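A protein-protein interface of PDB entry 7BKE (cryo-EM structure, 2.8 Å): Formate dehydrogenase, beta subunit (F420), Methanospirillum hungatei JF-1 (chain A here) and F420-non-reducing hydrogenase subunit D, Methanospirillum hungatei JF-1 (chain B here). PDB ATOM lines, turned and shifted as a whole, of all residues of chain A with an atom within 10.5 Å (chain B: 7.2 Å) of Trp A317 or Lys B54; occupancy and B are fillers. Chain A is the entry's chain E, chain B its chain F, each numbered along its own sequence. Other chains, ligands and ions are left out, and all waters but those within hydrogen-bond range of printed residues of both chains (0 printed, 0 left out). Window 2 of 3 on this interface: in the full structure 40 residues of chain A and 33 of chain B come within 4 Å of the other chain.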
ATOM      1  N   GLU A 310      28.636 -29.044 -10.810  1.00  0.00           N
ATOM      2  CA  GLU A 310      27.870 -28.160  -9.945  1.00  0.00           C
ATOM      3  C   GLU A 310      27.141 -27.153 -10.816  1.00  0.00           C
ATOM      4  O   GLU A 310      27.773 -26.437 -11.593  1.00  0.00           O
ATOM      5  CB  GLU A 310      28.770 -27.445  -8.944  1.00  0.00           C
ATOM      6  CG  GLU A 310      28.017 -26.579  -7.977  1.00  0.00           C
ATOM      7  CD  GLU A 310      28.936 -25.869  -7.020  1.00  0.00           C
ATOM      8  OE1 GLU A 310      30.161 -26.066  -7.126  1.00  0.00           O
ATOM      9  OE2 GLU A 310      28.441 -25.106  -6.166  1.00  0.00           O
ATOM     10  N   CYS A 311      25.842 -27.046 -10.637  1.00  0.00           N
ATOM     11  CA  CYS A 311      25.064 -26.091 -11.425  1.00  0.00           C
ATOM     12  C   CYS A 311      25.416 -24.679 -10.985  1.00  0.00           C
ATOM     13  O   CYS A 311      25.698 -24.486  -9.832  1.00  0.00           O
ATOM     14  CB  CYS A 311      23.583 -26.424 -11.329  1.00  0.00           C
ATOM     15  SG  CYS A 311      22.479 -25.560 -12.456  1.00  0.00           S
ATOM     16  N   SER A 312      25.380 -23.735 -11.905  1.00  0.00           N
ATOM     17  CA  SER A 312      25.576 -22.326 -11.561  1.00  0.00           C
ATOM     18  C   SER A 312      24.385 -21.878 -10.738  1.00  0.00           C
ATOM     19  O   SER A 312      24.519 -20.902 -10.033  1.00  0.00           O
ATOM     20  CB  SER A 312      25.709 -21.561 -12.797  1.00  0.00           C
ATOM     21  OG  SER A 312      26.887 -21.933 -13.484  1.00  0.00           O
ATOM     22  N   THR A 313      23.265 -22.583 -10.790  1.00  0.00           N
ATOM     23  CA  THR A 313      22.187 -22.208  -9.889  1.00  0.00           C
ATOM     24  C   THR A 313      22.530 -22.472  -8.432  1.00  0.00           C
ATOM     25  O   THR A 313      21.775 -22.057  -7.551  1.00  0.00           O
ATOM     26  CB  THR A 313      20.913 -22.958 -10.258  1.00  0.00           C
ATOM     27  OG1 THR A 313      21.188 -24.355 -10.332  1.00  0.00           O
ATOM     28  CG2 THR A 313      20.406 -22.507 -11.600  1.00  0.00           C
ATOM     29  N   LYS A 314      23.636 -23.158  -8.162  1.00  0.00           N
ATOM     30  CA  LYS A 314      24.073 -23.456  -6.808  1.00  0.00           C
ATOM     31  C   LYS A 314      25.192 -22.551  -6.325  1.00  0.00           C
ATOM     32  O   LYS A 314      25.652 -22.710  -5.195  1.00  0.00           O
ATOM     33  CB  LYS A 314      24.532 -24.910  -6.719  1.00  0.00           C
ATOM     34  CG  LYS A 314      23.412 -25.902  -6.565  1.00  0.00           C
ATOM     35  CD  LYS A 314      23.709 -27.164  -7.325  1.00  0.00           C
ATOM     36  CE  LYS A 314      22.914 -28.318  -6.781  1.00  0.00           C
ATOM     37  NZ  LYS A 314      23.073 -29.534  -7.610  1.00  0.00           N
ATOM     38  N   LYS A 315      25.631 -21.629  -7.125  1.00  0.00           N
ATOM     39  CA  LYS A 315      26.771 -20.798  -6.768  1.00  0.00           C
ATOM     40  C   LYS A 315      26.297 -19.541  -6.055  1.00  0.00           C
ATOM     41  O   LYS A 315      25.396 -18.863  -6.551  1.00  0.00           O
ATOM     42  CB  LYS A 315      27.565 -20.443  -8.007  1.00  0.00           C
ATOM     43  CG  LYS A 315      27.999 -21.674  -8.748  1.00  0.00           C
ATOM     44  CD  LYS A 315      28.933 -21.376  -9.878  1.00  0.00           C
ATOM     45  CE  LYS A 315      29.466 -22.654 -10.469  1.00  0.00           C
ATOM     46  NZ  LYS A 315      29.602 -23.681  -9.421  1.00  0.00           N
ATOM     47  N   PRO A 316      26.871 -19.211  -4.900  1.00  0.00           N
ATOM     48  CA  PRO A 316      26.285 -18.160  -4.062  1.00  0.00           C
ATOM     49  C   PRO A 316      26.335 -16.777  -4.671  1.00  0.00           C
ATOM     50  O   PRO A 316      25.615 -15.893  -4.196  1.00  0.00           O
ATOM     51  CB  PRO A 316      27.123 -18.231  -2.784  1.00  0.00           C
ATOM     52  CG  PRO A 316      28.402 -18.802  -3.217  1.00  0.00           C
ATOM     53  CD  PRO A 316      28.090 -19.772  -4.302  1.00  0.00           C
ATOM     54  N   TRP A 317      27.156 -16.543  -5.687  1.00  0.00           N
ATOM     55  CA  TRP A 317      27.157 -15.233  -6.317  1.00  0.00           C
ATOM     56  C   TRP A 317      26.064 -15.078  -7.362  1.00  0.00           C
ATOM     57  O   TRP A 317      25.860 -13.971  -7.858  1.00  0.00           O
ATOM     58  CB  TRP A 317      28.513 -14.943  -6.942  1.00  0.00           C
ATOM     59  CG  TRP A 317      29.066 -16.028  -7.779  1.00  0.00           C
ATOM     60  CD1 TRP A 317      28.877 -16.206  -9.103  1.00  0.00           C
ATOM     61  CD2 TRP A 317      29.944 -17.068  -7.353  1.00  0.00           C
ATOM     62  NE1 TRP A 317      29.568 -17.304  -9.536  1.00  0.00           N
ATOM     63  CE2 TRP A 317      30.233 -17.850  -8.475  1.00  0.00           C
ATOM     64  CE3 TRP A 317      30.508 -17.416  -6.129  1.00  0.00           C
ATOM     65  CZ2 TRP A 317      31.056 -18.958  -8.413  1.00  0.00           C
ATOM     66  CZ3 TRP A 317      31.318 -18.512  -6.070  1.00  0.00           C
ATOM     67  CH2 TRP A 317      31.589 -19.272  -7.200  1.00  0.00           C
ATOM     68  N   TYR A 318      25.348 -16.148  -7.696  1.00  0.00           N
ATOM     69  CA  TYR A 318      24.181 -16.065  -8.559  1.00  0.00           C
ATOM     70  C   TYR A 318      22.882 -16.151  -7.774  1.00  0.00           C
ATOM     71  O   TYR A 318      21.999 -15.312  -7.945  1.00  0.00           O
ATOM     72  CB  TYR A 318      24.218 -17.174  -9.607  1.00  0.00           C
ATOM     73  CG  TYR A 318      25.206 -16.943 -10.708  1.00  0.00           C
ATOM     74  CD1 TYR A 318      25.325 -15.706 -11.307  1.00  0.00           C
ATOM     75  CD2 TYR A 318      26.022 -17.962 -11.152  1.00  0.00           C
ATOM     76  CE1 TYR A 318      26.228 -15.492 -12.310  1.00  0.00           C
ATOM     77  CE2 TYR A 318      26.924 -17.761 -12.154  1.00  0.00           C
ATOM     78  CZ  TYR A 318      27.024 -16.526 -12.731  1.00  0.00           C
ATOM     79  OH  TYR A 318      27.928 -16.327 -13.739  1.00  0.00           O
ATOM     80  N   ILE A 319      22.754 -17.149  -6.908  1.00  0.00           N
ATOM     81  CA  ILE A 319      21.532 -17.407  -6.158  1.00  0.00           C
ATOM     82  C   ILE A 319      21.861 -17.398  -4.673  1.00  0.00           C
ATOM     83  O   ILE A 319      22.750 -18.129  -4.226  1.00  0.00           O
ATOM     84  CB  ILE A 319      20.899 -18.747  -6.564  1.00  0.00           C
ATOM     85  CG1 ILE A 319      20.672 -18.796  -8.072  1.00  0.00           C
ATOM     86  CG2 ILE A 319      19.605 -18.971  -5.817  1.00  0.00           C
ATOM     87  CD1 ILE A 319      19.448 -18.087  -8.519  1.00  0.00           C
ATOM     88  N   ALA A 320      21.138 -16.589  -3.915  1.00  0.00           N
ATOM     89  CA  ALA A 320      21.335 -16.545  -2.470  1.00  0.00           C
ATOM     90  C   ALA A 320      20.934 -17.878  -1.851  1.00  0.00           C
ATOM     91  O   ALA A 320      19.817 -18.352  -2.082  1.00  0.00           O
ATOM     92  CB  ALA A 320      20.527 -15.410  -1.859  1.00  0.00           C
ATOM     93  N   PRO A 321      21.803 -18.503  -1.050  1.00  0.00           N
ATOM     94  CA  PRO A 321      21.567 -19.905  -0.663  1.00  0.00           C
ATOM     95  C   PRO A 321      20.281 -20.155   0.100  1.00  0.00           C
ATOM     96  O   PRO A 321      19.656 -21.206  -0.090  1.00  0.00           O
ATOM     97  CB  PRO A 321      22.799 -20.227   0.197  1.00  0.00           C
ATOM     98  CG  PRO A 321      23.819 -19.230  -0.206  1.00  0.00           C
ATOM     99  CD  PRO A 321      23.064 -17.987  -0.506  1.00  0.00           C
ATOM    100  N   GLY A 322      19.864 -19.240   0.965  1.00  0.00           N
ATOM    101  CA  GLY A 322      18.753 -19.538   1.845  1.00  0.00           C
ATOM    102  C   GLY A 322      17.434 -18.897   1.474  1.00  0.00           C
ATOM    103  O   GLY A 322      16.385 -19.284   1.993  1.00  0.00           O
ATOM    104  N   THR A 326      12.752 -17.852  -4.607  1.00  0.00           N
ATOM    105  CA  THR A 326      14.003 -17.695  -5.326  1.00  0.00           C
ATOM    106  C   THR A 326      13.868 -16.710  -6.481  1.00  0.00           C
ATOM    107  O   THR A 326      12.775 -16.401  -6.956  1.00  0.00           O
ATOM    108  CB  THR A 326      14.483 -19.048  -5.844  1.00  0.00           C
ATOM    109  OG1 THR A 326      15.668 -18.868  -6.623  1.00  0.00           O
ATOM    110  CG2 THR A 326      13.427 -19.695  -6.695  1.00  0.00           C
ATOM    111  N   SER A 327      15.012 -16.213  -6.926  1.00  0.00           N
ATOM    112  CA  SER A 327      15.054 -15.220  -7.981  1.00  0.00           C
ATOM    113  C   SER A 327      14.670 -15.830  -9.322  1.00  0.00           C
ATOM    114  O   SER A 327      14.700 -17.045  -9.517  1.00  0.00           O
ATOM    115  CB  SER A 327      16.449 -14.609  -8.069  1.00  0.00           C
ATOM    116  OG  SER A 327      16.525 -13.673  -9.120  1.00  0.00           O
ATOM    117  N   PHE A 328      14.288 -14.962 -10.254  1.00  0.00           N
ATOM    118  CA  PHE A 328      14.104 -15.365 -11.638  1.00  0.00           C
ATOM    119  C   PHE A 328      15.417 -15.780 -12.276  1.00  0.00           C
ATOM    120  O   PHE A 328      15.409 -16.388 -13.353  1.00  0.00           O
ATOM    121  CB  PHE A 328      13.456 -14.219 -12.415  1.00  0.00           C
ATOM    122  CG  PHE A 328      12.925 -14.607 -13.755  1.00  0.00           C
ATOM    123  CD1 PHE A 328      13.017 -13.739 -14.818  1.00  0.00           C
ATOM    124  CD2 PHE A 328      12.332 -15.830 -13.954  1.00  0.00           C
ATOM    125  CE1 PHE A 328      12.539 -14.089 -16.053  1.00  0.00           C
ATOM    126  CE2 PHE A 328      11.851 -16.180 -15.190  1.00  0.00           C
ATOM    127  CZ  PHE A 328      11.957 -15.309 -16.239  1.00  0.00           C
ATOM    128  N   MET A 329      16.538 -15.470 -11.628  1.00  0.00           N
ATOM    129  CA  MET A 329      17.841 -15.865 -12.139  1.00  0.00           C
ATOM    130  C   MET A 329      17.967 -17.375 -12.230  1.00  0.00           C
ATOM    131  O   MET A 329      18.670 -17.884 -13.105  1.00  0.00           O
ATOM    132  CB  MET A 329      18.936 -15.288 -11.247  1.00  0.00           C
ATOM    133  CG  MET A 329      20.344 -15.452 -11.772  1.00  0.00           C
ATOM    134  SD  MET A 329      20.674 -14.310 -13.102  1.00  0.00           S
ATOM    135  CE  MET A 329      21.687 -15.299 -14.172  1.00  0.00           C
ATOM    136  N   PHE A 330      17.276 -18.109 -11.357  1.00  0.00           N
ATOM    137  CA  PHE A 330      17.337 -19.565 -11.386  1.00  0.00           C
ATOM    138  C   PHE A 330      16.910 -20.099 -12.742  1.00  0.00           C
ATOM    139  O   PHE A 330      17.556 -20.983 -13.305  1.00  0.00           O
ATOM    140  CB  PHE A 330      16.454 -20.148 -10.285  1.00  0.00           C
ATOM    141  CG  PHE A 330      16.606 -21.632 -10.095  1.00  0.00           C
ATOM    142  CD1 PHE A 330      17.245 -22.130  -8.987  1.00  0.00           C
ATOM    143  CD2 PHE A 330      16.088 -22.525 -11.009  1.00  0.00           C
ATOM    144  CE1 PHE A 330      17.376 -23.480  -8.815  1.00  0.00           C
ATOM    145  CE2 PHE A 330      16.228 -23.865 -10.840  1.00  0.00           C
ATOM    146  CZ  PHE A 330      16.865 -24.345  -9.746  1.00  0.00           C
ATOM    147  N   HIS A 331      15.818 -19.583 -13.276  1.00  0.00           N
ATOM    148  CA  HIS A 331      15.318 -20.057 -14.550  1.00  0.00           C
ATOM    149  C   HIS A 331      15.945 -19.343 -15.725  1.00  0.00           C
ATOM    150  O   HIS A 331      15.975 -19.901 -16.821  1.00  0.00           O
ATOM    151  CB  HIS A 331      13.805 -19.918 -14.588  1.00  0.00           C
ATOM    152  CG  HIS A 331      13.119 -20.793 -13.597  1.00  0.00           C
ATOM    153  ND1 HIS A 331      12.904 -20.408 -12.293  1.00  0.00           N
ATOM    154  CD2 HIS A 331      12.653 -22.057 -13.700  1.00  0.00           C
ATOM    155  CE1 HIS A 331      12.311 -21.390 -11.643  1.00  0.00           C
ATOM    156  NE2 HIS A 331      12.147 -22.401 -12.475  1.00  0.00           N
ATOM    157  N   LEU A 332      16.456 -18.132 -15.522  1.00  0.00           N
ATOM    158  CA  LEU A 332      17.226 -17.493 -16.577  1.00  0.00           C
ATOM    159  C   LEU A 332      18.508 -18.262 -16.861  1.00  0.00           C
ATOM    160  O   LEU A 332      18.927 -18.366 -18.015  1.00  0.00           O
ATOM    161  CB  LEU A 332      17.530 -16.053 -16.195  1.00  0.00           C
ATOM    162  CG  LEU A 332      16.346 -15.105 -16.284  1.00  0.00           C
ATOM    163  CD1 LEU A 332      16.772 -13.715 -15.909  1.00  0.00           C
ATOM    164  CD2 LEU A 332      15.801 -15.126 -17.679  1.00  0.00           C
ATOM    165  N   ILE A 333      19.106 -18.885 -15.844  1.00  0.00           N
ATOM    166  CA  ILE A 333      20.389 -19.626 -15.992  1.00  0.00           C
ATOM    167  C   ILE A 333      20.123 -20.912 -16.747  1.00  0.00           C
ATOM    168  O   ILE A 333      21.000 -21.327 -17.479  1.00  0.00           O
ATOM    169  CB  ILE A 333      21.013 -19.955 -14.621  1.00  0.00           C
ATOM    170  CG1 ILE A 333      21.563 -18.729 -13.898  1.00  0.00           C
ATOM    171  CG2 ILE A 333      22.070 -21.040 -14.721  1.00  0.00           C
ATOM    172  CD1 ILE A 333      21.903 -18.986 -12.453  1.00  0.00           C
ATOM    173  N   ALA A 336      19.388 -19.791 -20.498  1.00  0.00           N
ATOM    174  CA  ALA A 336      20.629 -19.472 -21.187  1.00  0.00           C
ATOM    175  C   ALA A 336      21.405 -20.724 -21.547  1.00  0.00           C
ATOM    176  O   ALA A 336      21.999 -20.801 -22.626  1.00  0.00           O
ATOM    177  CB  ALA A 336      21.476 -18.547 -20.324  1.00  0.00           C
ATOM    178  N   HIS A 337      21.437 -21.722 -20.668  1.00  0.00           N
ATOM    179  CA  HIS A 337      22.312 -22.900 -20.893  1.00  0.00           C
ATOM    180  C   HIS A 337      21.666 -24.012 -21.692  1.00  0.00           C
ATOM    181  O   HIS A 337      22.399 -24.731 -22.341  1.00  0.00           O
ATOM    182  CB  HIS A 337      22.773 -23.438 -19.552  1.00  0.00           C
ATOM    183  CG  HIS A 337      23.786 -22.617 -18.840  1.00  0.00           C
ATOM    184  ND1 HIS A 337      24.065 -22.813 -17.514  1.00  0.00           N
ATOM    185  CD2 HIS A 337      24.591 -21.623 -19.253  1.00  0.00           C
ATOM    186  CE1 HIS A 337      24.986 -21.962 -17.134  1.00  0.00           C
ATOM    187  NE2 HIS A 337      25.325 -21.230 -18.179  1.00  0.00           N
ATOM    188  N   MET B  49      26.945 -15.019 -20.664  1.00  0.00           N
ATOM    189  CA  MET B  49      25.532 -14.671 -20.725  1.00  0.00           C
ATOM    190  C   MET B  49      24.968 -14.369 -19.356  1.00  0.00           C
ATOM    191  O   MET B  49      24.077 -13.521 -19.219  1.00  0.00           O
ATOM    192  CB  MET B  49      24.742 -15.805 -21.336  1.00  0.00           C
ATOM    193  CG  MET B  49      25.066 -16.094 -22.739  1.00  0.00           C
ATOM    194  SD  MET B  49      24.354 -17.662 -23.159  1.00  0.00           S
ATOM    195  CE  MET B  49      24.420 -17.461 -24.905  1.00  0.00           C
ATOM    196  N   LEU B  50      25.432 -15.088 -18.346  1.00  0.00           N
ATOM    197  CA  LEU B  50      24.900 -14.900 -17.012  1.00  0.00           C
ATOM    198  C   LEU B  50      25.228 -13.527 -16.461  1.00  0.00           C
ATOM    199  O   LEU B  50      24.486 -13.038 -15.614  1.00  0.00           O
ATOM    200  CB  LEU B  50      25.411 -15.998 -16.091  1.00  0.00           C
ATOM    201  CG  LEU B  50      25.197 -17.429 -16.582  1.00  0.00           C
ATOM    202  CD1 LEU B  50      25.400 -18.396 -15.451  1.00  0.00           C
ATOM    203  CD2 LEU B  50      23.829 -17.634 -17.197  1.00  0.00           C
ATOM    204  N   PHE B  51      26.280 -12.869 -16.953  1.00  0.00           N
ATOM    205  CA  PHE B  51      26.532 -11.484 -16.561  1.00  0.00           C
ATOM    206  C   PHE B  51      25.400 -10.579 -17.019  1.00  0.00           C
ATOM    207  O   PHE B  51      24.866  -9.784 -16.242  1.00  0.00           O
ATOM    208  CB  PHE B  51      27.850 -10.993 -17.150  1.00  0.00           C
ATOM    209  CG  PHE B  51      29.055 -11.680 -16.607  1.00  0.00           C
ATOM    210  CD1 PHE B  51      28.984 -12.427 -15.457  1.00  0.00           C
ATOM    211  CD2 PHE B  51      30.263 -11.577 -17.255  1.00  0.00           C
ATOM    212  CE1 PHE B  51      30.092 -13.056 -14.970  1.00  0.00           C
ATOM    213  CE2 PHE B  51      31.369 -12.207 -16.769  1.00  0.00           C
ATOM    214  CZ  PHE B  51      31.283 -12.945 -15.624  1.00  0.00           C
ATOM    215  N   ILE B  52      25.027 -10.695 -18.292  1.00  0.00           N
ATOM    216  CA  ILE B  52      23.960  -9.871 -18.850  1.00  0.00           C
ATOM    217  C   ILE B  52      22.647 -10.155 -18.142  1.00  0.00           C
ATOM    218  O   ILE B  52      21.913  -9.238 -17.759  1.00  0.00           O
ATOM    219  CB  ILE B  52      23.844 -10.117 -20.363  1.00  0.00           C
ATOM    220  CG1 ILE B  52      25.218 -10.086 -21.010  1.00  0.00           C
ATOM    221  CG2 ILE B  52      22.929  -9.105 -20.991  1.00  0.00           C
ATOM    222  CD1 ILE B  52      25.951  -8.819 -20.772  1.00  0.00           C
ATOM    223  N   LEU B  53      22.331 -11.434 -17.965  1.00  0.00           N
ATOM    224  CA  LEU B  53      21.065 -11.789 -17.342  1.00  0.00           C
ATOM    225  C   LEU B  53      21.029 -11.360 -15.885  1.00  0.00           C
ATOM    226  O   LEU B  53      19.984 -10.933 -15.387  1.00  0.00           O
ATOM    227  CB  LEU B  53      20.818 -13.284 -17.482  1.00  0.00           C
ATOM    228  CG  LEU B  53      20.737 -13.728 -18.938  1.00  0.00           C
ATOM    229  CD1 LEU B  53      20.417 -15.194 -19.024  1.00  0.00           C
ATOM    230  CD2 LEU B  53      19.709 -12.915 -19.678  1.00  0.00           C
ATOM    231  N   LYS B  54      22.155 -11.466 -15.183  1.00  0.00           N
ATOM    232  CA  LYS B  54      22.234 -10.990 -13.812  1.00  0.00           C
ATOM    233  C   LYS B  54      22.010  -9.492 -13.744  1.00  0.00           C
ATOM    234  O   LYS B  54      21.307  -9.009 -12.855  1.00  0.00           O
ATOM    235  CB  LYS B  54      23.590 -11.365 -13.222  1.00  0.00           C
ATOM    236  CG  LYS B  54      23.829 -10.881 -11.818  1.00  0.00           C
ATOM    237  CD  LYS B  54      22.969 -11.621 -10.835  1.00  0.00           C
ATOM    238  CE  LYS B  54      23.571 -11.581  -9.459  1.00  0.00           C
ATOM    239  NZ  LYS B  54      22.533 -11.775  -8.426  1.00  0.00           N
ATOM    240  N   ALA B  55      22.595  -8.738 -14.670  1.00  0.00           N
ATOM    241  CA  ALA B  55      22.350  -7.301 -14.709  1.00  0.00           C
ATOM    242  C   ALA B  55      20.871  -7.006 -14.907  1.00  0.00           C
ATOM    243  O   ALA B  55      20.276  -6.199 -14.178  1.00  0.00           O
ATOM    244  CB  ALA B  55      23.172  -6.667 -15.822  1.00  0.00           C
ATOM    245  N   PHE B  56      20.252  -7.669 -15.880  1.00  0.00           N
ATOM    246  CA  PHE B  56      18.856  -7.391 -16.189  1.00  0.00           C
ATOM    247  C   PHE B  56      17.926  -7.813 -15.066  1.00  0.00           C
ATOM    248  O   PHE B  56      16.859  -7.220 -14.900  1.00  0.00           O
ATOM    249  CB  PHE B  56      18.453  -8.084 -17.480  1.00  0.00           C
ATOM    250  CG  PHE B  56      18.623  -7.235 -18.673  1.00  0.00           C
ATOM    251  CD1 PHE B  56      18.056  -5.983 -18.721  1.00  0.00           C
ATOM    252  CD2 PHE B  56      19.363  -7.670 -19.741  1.00  0.00           C
ATOM    253  CE1 PHE B  56      18.219  -5.196 -19.810  1.00  0.00           C
ATOM    254  CE2 PHE B  56      19.527  -6.884 -20.832  1.00  0.00           C
ATOM    255  CZ  PHE B  56      18.956  -5.648 -20.870  1.00  0.00           C
ATOM    256  N   VAL B  57      18.290  -8.843 -14.303  1.00  0.00           N
ATOM    257  CA  VAL B  57      17.432  -9.253 -13.201  1.00  0.00           C
ATOM    258  C   VAL B  57      17.697  -8.433 -11.947  1.00  0.00           C
ATOM    259  O   VAL B  57      16.810  -8.324 -11.098  1.00  0.00           O
ATOM    260  CB  VAL B  57      17.579 -10.754 -12.897  1.00  0.00           C
ATOM    261  CG1 VAL B  57      18.892 -11.038 -12.226  1.00  0.00           C
ATOM    262  CG2 VAL B  57      16.423 -11.243 -12.044  1.00  0.00           C
ATOM    263  N   GLU B  58      18.885  -7.853 -11.787  1.00  0.00           N
ATOM    264  CA  GLU B  58      19.058  -6.874 -10.721  1.00  0.00           C
ATOM    265  C   GLU B  58      18.375  -5.562 -11.030  1.00  0.00           C
ATOM    266  O   GLU B  58      18.088  -4.799 -10.104  1.00  0.00           O
ATOM    267  CB  GLU B  58      20.531  -6.599 -10.421  1.00  0.00           C
ATOM    268  CG  GLU B  58      21.341  -7.812 -10.100  1.00  0.00           C
ATOM    269  CD  GLU B  58      21.184  -8.211  -8.655  1.00  0.00           C
ATOM    270  OE1 GLU B  58      20.276  -7.676  -7.983  1.00  0.00           O
ATOM    271  OE2 GLU B  58      21.948  -9.081  -8.189  1.00  0.00           O
ATOM    272  N   GLY B  59      18.134  -5.266 -12.297  1.00  0.00           N
ATOM    273  CA  GLY B  59      17.317  -4.116 -12.591  1.00  0.00           C
ATOM    274  C   GLY B  59      17.927  -3.136 -13.561  1.00  0.00           C
ATOM    275  O   GLY B  59      17.533  -1.972 -13.581  1.00  0.00           O
ATOM    276  N   ALA B  60      18.886  -3.575 -14.360  1.00  0.00           N
ATOM    277  CA  ALA B  60      19.426  -2.706 -15.390  1.00  0.00           C
ATOM    278  C   ALA B  60      18.326  -2.306 -16.352  1.00  0.00           C
ATOM    279  O   ALA B  60      17.711  -3.161 -16.994  1.00  0.00           O
ATOM    280  CB  ALA B  60      20.553  -3.404 -16.142  1.00  0.00           C
ATOM    281  N   VAL B  63      21.535  -2.528 -20.913  1.00  0.00           N
ATOM    282  CA  VAL B  63      22.858  -3.134 -20.848  1.00  0.00           C
ATOM    283  C   VAL B  63      23.527  -2.922 -22.191  1.00  0.00           C
ATOM    284  O   VAL B  63      22.907  -3.128 -23.236  1.00  0.00           O
ATOM    285  CB  VAL B  63      22.793  -4.632 -20.497  1.00  0.00           C
ATOM    286  CG1 VAL B  63      24.134  -5.276 -20.687  1.00  0.00           C
ATOM    287  CG2 VAL B  63      22.343  -4.822 -19.072  1.00  0.00           C
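The side-chain amino group of Lys B54 lies within salt-bridge range of the side-chain carboxylate of Glu B58, 2.8 Å away.
The side-chain hydroxyl (OG) of Ser A327 lies close to the backbone NH (N) of Met A329, 3.1 Å away.
The backbone carbonyl oxygen of Ile A333 sits close to a ring nitrogen (ND1) of His A337 (3.4 Å).
Hydrophobic or aromatic side chains of chain B that line the printed part of chain A: Met B49, Leu B50, Leu B53 and Val B57.
Printed residues of chain A that touch a printed residue of chain B: Trp A317, Tyr A318, Ser A327, Met A329, Leu A332, Ala A336 and His A337.
Hydrophobic or aromatic side chains of chain A that line the printed part of chain B: Tyr A318, Met A329, Ala A336 and His A337.
Along chain A the printed residues that touch a printed residue of chain B span positions 317 to 337.
Among the printed residues, no Asp or Glu carboxylate lies within 4 Å of a Lys or Arg side-chain nitrogen of the other chain.
Trp A317 touches just one residue of chain B: Lys B54.
Printed residues of chain B within 4 Å of Ala A336: Met B49 and Leu B53.
Printed residues of chain A within 4 Å of Met B49: Ala A336.
Leu B53 touches just these residues of chain A: Met A329, Leu A332 and Ala A336.
Lys B54 touches just these residues of chain A: Trp A317, Tyr A318 and Met A329.
No residue of chain A comes within 4 Å of Ala B55.
Printed residues of chain A within 4 Å of Val B57: Ser A327 and Met A329.
The nearest residue of chain A that does not touch Lys B54 is Ile A319 (5.6 Å).
The nearest printed residue of chain B that does not touch Tyr A318 is Phe B51 (4.1 Å).
O of Trp A317 touches CE of Lys B54, at 3.7 Å.
O of Tyr A318 touches NZ of Lys B54, 3.6 Å away.
OG of Ser A327 touches CG2 of Val B57, at 3.8 Å.
CE of Met A329 touches O of Leu B50, at 3.9 Å.
CB of Leu B53 touches CE of Met A329, at 3.97 Å.
Met A329 touches Lys B54.
SD of Met A329 touches CG1 of Val B57 (3.8 Å).
Leu A332 touches Leu B53.
O of Ala A336 touches SD of Met B49 (3.96 Å).
Leu B53 touches Ala A336 (CD1 to CB, 3.7 Å).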
